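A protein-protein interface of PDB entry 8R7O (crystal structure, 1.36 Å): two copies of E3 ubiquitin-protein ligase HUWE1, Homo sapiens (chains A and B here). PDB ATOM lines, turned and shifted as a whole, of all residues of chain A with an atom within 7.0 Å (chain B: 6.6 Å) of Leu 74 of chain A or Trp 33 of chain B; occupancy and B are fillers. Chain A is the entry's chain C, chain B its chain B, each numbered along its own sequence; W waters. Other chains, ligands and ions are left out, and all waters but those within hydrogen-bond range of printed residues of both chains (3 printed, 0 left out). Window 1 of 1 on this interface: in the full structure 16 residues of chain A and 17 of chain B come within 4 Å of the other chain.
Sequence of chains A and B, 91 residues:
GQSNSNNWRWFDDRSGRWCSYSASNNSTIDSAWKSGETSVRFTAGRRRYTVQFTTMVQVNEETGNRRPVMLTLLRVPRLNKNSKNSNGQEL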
ATOM      1  N   ASN A   7      15.156 -11.780 -11.563  1.00  0.00           N
ATOM      2  CA  ASN A   7      16.133 -12.757 -11.134  1.00  0.00           C
ATOM      3  C   ASN A   7      17.507 -12.158 -10.877  1.00  0.00           C
ATOM      4  O   ASN A   7      18.310 -12.805 -10.197  1.00  0.00           O
ATOM      5  CB  ASN A   7      16.214 -13.922 -12.146  1.00  0.00           C
ATOM      6  CG  ASN A   7      16.519 -13.454 -13.564  1.00  0.00           C
ATOM      7  OD1 ASN A   7      16.118 -12.350 -13.990  1.00  0.00           O
ATOM      8  ND2 ASN A   7      17.274 -14.281 -14.300  1.00  0.00           N
ATOM      9  N   THR A  72      20.059 -14.878  -9.425  1.00  0.00           N
ATOM     10  CA  THR A  72      19.435 -15.883  -8.602  1.00  0.00           C
ATOM     11  C   THR A  72      19.235 -17.162  -9.420  1.00  0.00           C
ATOM     12  O   THR A  72      19.188 -17.141 -10.663  1.00  0.00           O
ATOM     13  CB  THR A  72      18.123 -15.363  -7.992  1.00  0.00           C
ATOM     14  OG1 THR A  72      17.214 -15.012  -9.027  1.00  0.00           O
ATOM     15  CG2 THR A  72      18.374 -14.090  -7.156  1.00  0.00           C
ATOM     16  N   LEU A  73      19.256 -18.291  -8.737  1.00  0.00           N
ATOM     17  CA  LEU A  73      19.046 -19.584  -9.360  1.00  0.00           C
ATOM     18  C   LEU A  73      17.892 -20.255  -8.657  1.00  0.00           C
ATOM     19  O   LEU A  73      17.918 -20.376  -7.428  1.00  0.00           O
ATOM     20  CB  LEU A  73      20.248 -20.469  -9.139  1.00  0.00           C
ATOM     21  CG  LEU A  73      21.494 -19.945  -9.784  1.00  0.00           C
ATOM     22  CD1 LEU A  73      22.537 -20.978  -9.487  1.00  0.00           C
ATOM     23  CD2 LEU A  73      21.256 -19.718 -11.267  1.00  0.00           C
ATOM     24  N   LEU A  74      16.972 -20.835  -9.456  1.00  0.00           N
ATOM     25  CA  LEU A  74      15.846 -21.606  -8.955  1.00  0.00           C
ATOM     26  C   LEU A  74      16.220 -23.088  -8.877  1.00  0.00           C
ATOM     27  O   LEU A  74      16.982 -23.618  -9.700  1.00  0.00           O
ATOM     28  CB  LEU A  74      14.649 -21.436  -9.889  1.00  0.00           C
ATOM     29  CG  LEU A  74      14.224 -19.962 -10.074  1.00  0.00           C
ATOM     30  CD1 LEU A  74      13.084 -19.806 -11.061  1.00  0.00           C
ATOM     31  CD2 LEU A  74      13.941 -19.247  -8.758  1.00  0.00           C
ATOM     32  N   ARG A  75      15.653 -23.762  -7.885  1.00  0.00           N
ATOM     33  CA  ARG A  75      15.973 -25.159  -7.639  1.00  0.00           C
ATOM     34  C   ARG A  75      15.574 -26.041  -8.816  1.00  0.00           C
ATOM     35  O   ARG A  75      14.502 -25.870  -9.410  1.00  0.00           O
ATOM     36  CB  ARG A  75      15.206 -25.595  -6.395  1.00  0.00           C
ATOM     37  CG  ARG A  75      15.621 -26.907  -5.796  1.00  0.00           C
ATOM     38  CD  ARG A  75      14.600 -27.355  -4.772  1.00  0.00           C
ATOM     39  NE  ARG A  75      15.053 -28.523  -4.021  1.00  0.00           N
ATOM     40  CZ  ARG A  75      14.934 -29.777  -4.430  1.00  0.00           C
ATOM     41  NH1 ARG A  75      14.462 -30.074  -5.632  1.00  0.00           N
ATOM     42  NH2 ARG A  75      15.294 -30.758  -3.610  1.00  0.00           N
ATOM     43  N   VAL A  76      16.411 -27.037  -9.117  1.00  0.00           N
ATOM     44  CA  VAL A  76      16.102 -28.054 -10.116  1.00  0.00           C
ATOM     45  C   VAL A  76      16.298 -29.421  -9.477  1.00  0.00           C
ATOM     46  O   VAL A  76      17.397 -29.719  -8.979  1.00  0.00           O
ATOM     47  CB  VAL A  76      16.981 -27.960 -11.377  1.00  0.00           C
ATOM     48  CG1 VAL A  76      16.629 -29.101 -12.390  1.00  0.00           C
ATOM     49  CG2 VAL A  76      16.836 -26.575 -11.989  1.00  0.00           C
ATOM     50  N   PRO A  77      15.273 -30.277  -9.442  1.00  0.00           N
ATOM     51  CA  PRO A  77      13.899 -30.036  -9.911  1.00  0.00           C
ATOM     52  C   PRO A  77      13.180 -29.066  -8.978  1.00  0.00           C
ATOM     53  O   PRO A  77      13.650 -28.732  -7.877  1.00  0.00           O
ATOM     54  CB  PRO A  77      13.230 -31.427  -9.790  1.00  0.00           C
ATOM     55  CG  PRO A  77      14.339 -32.390  -9.745  1.00  0.00           C
ATOM     56  CD  PRO A  77      15.441 -31.676  -9.002  1.00  0.00           C
ATOM     57  N   ARG A  78      11.991 -28.631  -9.383  1.00  0.00           N
ATOM     58  CA  ARG A  78      11.149 -27.775  -8.564  1.00  0.00           C
ATOM     59  C   ARG A  78      10.460 -28.584  -7.463  1.00  0.00           C
ATOM     60  O   ARG A  78      10.105 -29.753  -7.652  1.00  0.00           O
ATOM     61  CB  ARG A  78      10.102 -27.126  -9.474  1.00  0.00           C
ATOM     62  CG  ARG A  78       9.127 -26.219  -8.778  1.00  0.00           C
ATOM     63  CD  ARG A  78       8.723 -25.069  -9.708  1.00  0.00           C
ATOM     64  NE  ARG A  78       9.894 -24.257 -10.009  1.00  0.00           N
ATOM     65  CZ  ARG A  78       9.905 -23.276 -10.906  1.00  0.00           C
ATOM     66  NH1 ARG A  78       8.823 -22.987 -11.627  1.00  0.00           N
ATOM     67  NH2 ARG A  78      11.024 -22.572 -11.089  1.00  0.00           N
ATOM     68  N   ASN B   7      17.156 -22.501 -24.224  1.00  0.00           N
ATOM     69  CA  ASN B   7      17.751 -23.016 -23.021  1.00  0.00           C
ATOM     70  C   ASN B   7      17.123 -24.306 -22.529  1.00  0.00           C
ATOM     71  O   ASN B   7      17.786 -25.028 -21.779  1.00  0.00           O
ATOM     72  CB  ASN B   7      17.824 -21.968 -21.925  1.00  0.00           C
ATOM     73  CG  ASN B   7      16.468 -21.378 -21.576  1.00  0.00           C
ATOM     74  OD1 ASN B   7      15.584 -21.235 -22.432  1.00  0.00           O
ATOM     75  ND2 ASN B   7      16.291 -21.039 -20.293  1.00  0.00           N
ATOM     76  N   TRP B   8      15.898 -24.670 -22.958  1.00  0.00           N
ATOM     77  CA  TRP B   8      15.297 -25.925 -22.530  1.00  0.00           C
ATOM     78  C   TRP B   8      15.514 -26.984 -23.590  1.00  0.00           C
ATOM     79  O   TRP B   8      15.590 -26.683 -24.795  1.00  0.00           O
ATOM     80  CB  TRP B   8      13.790 -25.764 -22.287  1.00  0.00           C
ATOM     81  CG  TRP B   8      13.556 -25.038 -21.045  1.00  0.00           C
ATOM     82  CD1 TRP B   8      13.516 -23.671 -20.889  1.00  0.00           C
ATOM     83  CD2 TRP B   8      13.320 -25.600 -19.751  1.00  0.00           C
ATOM     84  NE1 TRP B   8      13.284 -23.348 -19.559  1.00  0.00           N
ATOM     85  CE2 TRP B   8      13.138 -24.518 -18.851  1.00  0.00           C
ATOM     86  CE3 TRP B   8      13.279 -26.900 -19.251  1.00  0.00           C
ATOM     87  CZ2 TRP B   8      12.908 -24.710 -17.496  1.00  0.00           C
ATOM     88  CZ3 TRP B   8      13.010 -27.076 -17.895  1.00  0.00           C
ATOM     89  CH2 TRP B   8      12.862 -25.986 -17.034  1.00  0.00           C
ATOM     90  N   THR B  28       7.348 -20.368 -23.869  1.00  0.00           N
ATOM     91  CA  THR B  28       6.219 -20.755 -23.032  1.00  0.00           C
ATOM     92  C   THR B  28       6.714 -21.509 -21.803  1.00  0.00           C
ATOM     93  O   THR B  28       6.328 -21.202 -20.663  1.00  0.00           O
ATOM     94  CB  THR B  28       5.245 -21.617 -23.852  1.00  0.00           C
ATOM     95  OG1 THR B  28       4.693 -20.834 -24.918  1.00  0.00           O
ATOM     96  CG2 THR B  28       4.081 -22.112 -22.990  1.00  0.00           C
ATOM     97  N   ILE B  29       7.629 -22.450 -22.022  1.00  0.00           N
ATOM     98  CA  ILE B  29       8.186 -23.237 -20.928  1.00  0.00           C
ATOM     99  C   ILE B  29       8.992 -22.347 -19.994  1.00  0.00           C
ATOM    100  O   ILE B  29       8.839 -22.414 -18.770  1.00  0.00           O
ATOM    101  CB  ILE B  29       9.030 -24.395 -21.487  1.00  0.00           C
ATOM    102  CG1 ILE B  29       8.152 -25.407 -22.223  1.00  0.00           C
ATOM    103  CG2 ILE B  29       9.801 -25.077 -20.366  1.00  0.00           C
ATOM    104  CD1 ILE B  29       8.983 -26.344 -23.048  1.00  0.00           C
ATOM    105  N   ASP B  30       9.866 -21.507 -20.555  1.00  0.00           N
ATOM    106  CA  ASP B  30      10.754 -20.720 -19.702  1.00  0.00           C
ATOM    107  C   ASP B  30       9.989 -19.678 -18.914  1.00  0.00           C
ATOM    108  O   ASP B  30      10.378 -19.337 -17.793  1.00  0.00           O
ATOM    109  CB  ASP B  30      11.842 -20.038 -20.525  1.00  0.00           C
ATOM    110  CG  ASP B  30      13.025 -19.634 -19.678  1.00  0.00           C
ATOM    111  OD1 ASP B  30      13.522 -20.510 -18.935  1.00  0.00           O
ATOM    112  OD2 ASP B  30      13.469 -18.467 -19.752  1.00  0.00           O
ATOM    113  N   SER B  31       8.921 -19.135 -19.486  1.00  0.00           N
ATOM    114  CA  SER B  31       8.140 -18.164 -18.738  1.00  0.00           C
ATOM    115  C   SER B  31       7.438 -18.820 -17.557  1.00  0.00           C
ATOM    116  O   SER B  31       7.331 -18.221 -16.471  1.00  0.00           O
ATOM    117  CB  SER B  31       7.125 -17.492 -19.654  1.00  0.00           C
ATOM    118  OG  SER B  31       6.263 -16.656 -18.898  1.00  0.00           O
ATOM    119  N   ALA B  32       6.943 -20.045 -17.756  1.00  0.00           N
ATOM    120  CA  ALA B  32       6.325 -20.770 -16.652  1.00  0.00           C
ATOM    121  C   ALA B  32       7.364 -21.122 -15.598  1.00  0.00           C
ATOM    122  O   ALA B  32       7.104 -20.990 -14.389  1.00  0.00           O
ATOM    123  CB  ALA B  32       5.597 -22.005 -17.178  1.00  0.00           C
ATOM    124  N   TRP B  33       8.556 -21.523 -16.034  1.00  0.00           N
ATOM    125  CA  TRP B  33       9.630 -21.789 -15.082  1.00  0.00           C
ATOM    126  C   TRP B  33       9.885 -20.565 -14.208  1.00  0.00           C
ATOM    127  O   TRP B  33       9.857 -20.640 -12.972  1.00  0.00           O
ATOM    128  CB  TRP B  33      10.901 -22.166 -15.843  1.00  0.00           C
ATOM    129  CG  TRP B  33      12.101 -22.406 -14.917  1.00  0.00           C
ATOM    130  CD1 TRP B  33      13.183 -21.590 -14.740  1.00  0.00           C
ATOM    131  CD2 TRP B  33      12.284 -23.516 -14.035  1.00  0.00           C
ATOM    132  NE1 TRP B  33      14.061 -22.156 -13.832  1.00  0.00           N
ATOM    133  CE2 TRP B  33      13.515 -23.323 -13.368  1.00  0.00           C
ATOM    134  CE3 TRP B  33      11.544 -24.682 -13.771  1.00  0.00           C
ATOM    135  CZ2 TRP B  33      14.028 -24.256 -12.464  1.00  0.00           C
ATOM    136  CZ3 TRP B  33      12.042 -25.594 -12.869  1.00  0.00           C
ATOM    137  CH2 TRP B  33      13.282 -25.363 -12.207  1.00  0.00           C
ATOM    138  N   LYS B  34      10.044 -19.409 -14.841  1.00  0.00           N
ATOM    139  CA  LYS B  34      10.414 -18.198 -14.116  1.00  0.00           C
ATOM    140  C   LYS B  34       9.298 -17.732 -13.182  1.00  0.00           C
ATOM    141  O   LYS B  34       9.572 -17.053 -12.180  1.00  0.00           O
ATOM    142  CB  LYS B  34      10.705 -17.078 -15.119  1.00  0.00           C
ATOM    143  CG  LYS B  34      11.928 -17.252 -16.001  1.00  0.00           C
ATOM    144  CD  LYS B  34      13.220 -17.376 -15.269  1.00  0.00           C
ATOM    145  CE  LYS B  34      14.291 -16.566 -16.026  1.00  0.00           C
ATOM    146  NZ  LYS B  34      15.648 -17.167 -16.023  1.00  0.00           N
ATOM    147  N   SER B  35       8.040 -18.047 -13.496  1.00  0.00           N
ATOM    148  CA  SER B  35       6.933 -17.590 -12.662  1.00  0.00           C
ATOM    149  C   SER B  35       6.643 -18.517 -11.493  1.00  0.00           C
ATOM    150  O   SER B  35       5.677 -18.277 -10.762  1.00  0.00           O
ATOM    151  CB  SER B  35       5.663 -17.397 -13.495  1.00  0.00           C
ATOM    152  OG  SER B  35       5.266 -18.609 -14.101  1.00  0.00           O
ATOM    153  N   GLY B  36       7.437 -19.567 -11.306  1.00  0.00           N
ATOM    154  CA  GLY B  36       7.248 -20.466 -10.182  1.00  0.00           C
ATOM    155  C   GLY B  36       6.179 -21.516 -10.366  1.00  0.00           C
ATOM    156  O   GLY B  36       5.856 -22.214  -9.393  1.00  0.00           O
ATOM    157  N   GLU B  37       5.631 -21.663 -11.571  1.00  0.00           N
ATOM    158  CA  GLU B  37       4.597 -22.669 -11.796  1.00  0.00           C
ATOM    159  C   GLU B  37       5.209 -24.064 -11.643  1.00  0.00           C
ATOM    160  O   GLU B  37       6.396 -24.278 -11.912  1.00  0.00           O
ATOM    161  CB  GLU B  37       4.118 -22.611 -13.249  1.00  0.00           C
ATOM    162  CG  GLU B  37       3.569 -21.275 -13.770  1.00  0.00           C
ATOM    163  CD  GLU B  37       2.314 -20.801 -13.089  1.00  0.00           C
ATOM    164  OE1 GLU B  37       1.978 -21.286 -11.980  1.00  0.00           O
ATOM    165  OE2 GLU B  37       1.596 -20.000 -13.728  1.00  0.00           O
ATOM    166  N   VAL B  40       3.626 -26.806 -16.974  1.00  0.00           N
ATOM    167  CA  VAL B  40       3.199 -25.939 -18.062  1.00  0.00           C
ATOM    168  C   VAL B  40       2.737 -26.795 -19.227  1.00  0.00           C
ATOM    169  O   VAL B  40       3.302 -27.857 -19.507  1.00  0.00           O
ATOM    170  CB  VAL B  40       4.349 -25.006 -18.475  1.00  0.00           C
ATOM    171  CG1 VAL B  40       5.589 -25.815 -18.930  1.00  0.00           C
ATOM    172  CG2 VAL B  40       3.874 -23.978 -19.522  1.00  0.00           C
ATOM    173  N   PHE B  53       7.627 -29.673 -13.912  1.00  0.00           N
ATOM    174  CA  PHE B  53       8.875 -29.170 -13.367  1.00  0.00           C
ATOM    175  C   PHE B  53       9.289 -29.877 -12.077  1.00  0.00           C
ATOM    176  O   PHE B  53      10.472 -29.817 -11.706  1.00  0.00           O
ATOM    177  CB  PHE B  53       8.724 -27.677 -13.113  1.00  0.00           C
ATOM    178  CG  PHE B  53       8.608 -26.832 -14.378  1.00  0.00           C
ATOM    179  CD1 PHE B  53       9.457 -27.019 -15.472  1.00  0.00           C
ATOM    180  CD2 PHE B  53       7.669 -25.818 -14.445  1.00  0.00           C
ATOM    181  CE1 PHE B  53       9.366 -26.219 -16.598  1.00  0.00           C
ATOM    182  CE2 PHE B  53       7.582 -24.979 -15.559  1.00  0.00           C
ATOM    183  CZ  PHE B  53       8.407 -25.209 -16.660  1.00  0.00           C
ATOM    184  N   THR B  54       8.354 -30.516 -11.365  1.00  0.00           N
ATOM    185  CA  THR B  54       8.723 -31.189 -10.129  1.00  0.00           C
ATOM    186  C   THR B  54       9.404 -32.514 -10.421  1.00  0.00           C
ATOM    187  O   THR B  54      10.138 -33.024  -9.561  1.00  0.00           O
ATOM    188  CB  THR B  54       7.501 -31.430  -9.244  1.00  0.00           C
ATOM    189  OG1 THR B  54       6.562 -32.249  -9.956  1.00  0.00           O
ATOM    190  CG2 THR B  54       6.846 -30.071  -8.831  1.00  0.00           C
ATOM    191  N   MET B  56      10.853 -32.898 -13.832  1.00  0.00           N
ATOM    192  CA  MET B  56      11.685 -32.628 -14.998  1.00  0.00           C
ATOM    193  C   MET B  56      11.398 -33.627 -16.109  1.00  0.00           C
ATOM    194  O   MET B  56      12.308 -34.234 -16.682  1.00  0.00           O
ATOM    195  CB  MET B  56      13.175 -32.556 -14.652  1.00  0.00           C
ATOM    196  CG  MET B  56      13.453 -31.396 -13.671  1.00  0.00           C
ATOM    197  SD  MET B  56      13.092 -29.751 -14.288  1.00  0.00           S
ATOM    198  CE  MET B  56      14.499 -29.530 -15.374  1.00  0.00           C
ATOM    199  N   LEU B  71      17.289 -28.076 -18.212  1.00  0.00           N
ATOM    200  CA  LEU B  71      17.488 -26.652 -18.349  1.00  0.00           C
ATOM    201  C   LEU B  71      18.988 -26.419 -18.485  1.00  0.00           C
ATOM    202  O   LEU B  71      19.772 -26.805 -17.607  1.00  0.00           O
ATOM    203  CB  LEU B  71      16.931 -25.956 -17.097  1.00  0.00           C
ATOM    204  CG  LEU B  71      17.204 -24.495 -16.899  1.00  0.00           C
ATOM    205  CD1 LEU B  71      16.712 -23.716 -18.110  1.00  0.00           C
ATOM    206  CD2 LEU B  71      16.482 -24.061 -15.650  1.00  0.00           C
HETATM  207  O   HOH W   1      16.801 -20.517 -12.593  1.00  0.00           O
HETATM  208  O   HOH W   2      17.847 -16.023 -17.021  1.00  0.00           O
HETATM  209  O   HOH W   3      10.485 -32.269  -6.753  1.00  0.00           O
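Water W2 bridges the side-chain amino group (NZ) of Lys 34 of chain B and the side-chain amide nitrogen (ND2) of Asn 7 of chain A. Water W3 lies within hydrogen-bond range of O of Arg 78 of chain A and O of Thr 54 of chain B. Water W1 bridges N of Leu 74 of chain A (3.2 Å) and NE1 of Trp 33 of chain B (3.4 Å).
Leu 74 of chain A touches one residue of chain B. Trp 33 of chain B touches just these residues of chain A: Leu 74 (3.8 Å), Arg 75 (3.1 Å), Val 76 (3.7 Å) and Arg 78 (2.9 Å). Of the printed residues of chain B, Arg 78 of chain A touches Ala 32, Trp 33, Gly 36, Glu 37, Phe 53 and Thr 54. Of the printed residues of chain A, Glu 37 of chain B touches Arg 78 (2.8 Å). Of the printed residues of chain B, Val 76 of chain A touches Trp 33 and Met 56. Printed residues of chain A within 4 Å of Gly 36 of chain B: Arg 78. Thr 28 of chain B touches none of the printed residues of chain A. The nearest residue of chain B that does not touch Leu 74 of chain A is Lys 34 of chain B (4.4 Å). The nearest residue of chain A that does not touch Trp 33 of chain B is Pro 77 of chain A (4.9 Å).
Among the printed residues, pairs that only touch across the chains: Asn 7 of chain A with Lys 34 of chain B, Leu 74 of chain A with Trp 33 of chain B, Arg 75 of chain A with Trp 33 of chain B, Val 76 of chain A with Trp 33 of chain B, Val 76 of chain A with Met 56 of chain B, Pro 77 of chain A with Phe 53 of chain B, Pro 77 of chain A with Thr 54 of chain B, Pro 77 of chain A with Met 56 of chain B, Arg 78 of chain A with Ala 32 of chain B, Arg 78 of chain A with Gly 36 of chain B and Arg 78 of chain A with Thr 54 of chain B.
Hydrophobic or aromatic side chains of chain B within 4 Å of the printed part of chain A: Trp 33, Phe 53 and Met 56. Along chain B the printed residues that touch a printed residue of chain A span positions 32 to 56. Of the 8 printed residues of chain A, 6 touch a printed residue of chain B. Printed residues of chain A that touch a printed residue of chain B: Asn 7, Leu 74, Arg 75, Val 76, Pro 77 and Arg 78. Hydrophobic or aromatic side chains of chain A that line the printed part of chain B: Leu 74, Val 76 and Pro 77.
O of Trp 33 of chain B lies within hydrogen-bond range of NH1 of Arg 78 of chain A, 2.9 Å away. NH1 of Arg 78 of chain A lies within hydrogen-bond range of O of Glu 37 of chain B (2.8 Å). O of Phe 53 of chain B lies within hydrogen-bond range of N of Arg 78 of chain A (3.0 Å).
The backbone carbonyl oxygen (O) of Ala 32 of chain B lies within hydrogen-bond range of the side-chain hydroxyl (OG) of Ser 35 of chain B. N of Glu 37 of chain B lies within hydrogen-bond range of O of Ala 32 of chain B, at 3.3 Å. The backbone carbonyl oxygen (O) of Asn 7 of chain A lies within hydrogen-bond range of the side-chain hydroxyl (OG1) of Thr 72 of chain A (2.7 Å). The backbone carbonyl oxygen (O) of Pro 77 of chain A lies within hydrogen-bond range of the guanidinium group (NH1) of Arg 75 of chain A.
Position printed for both chains: 7.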
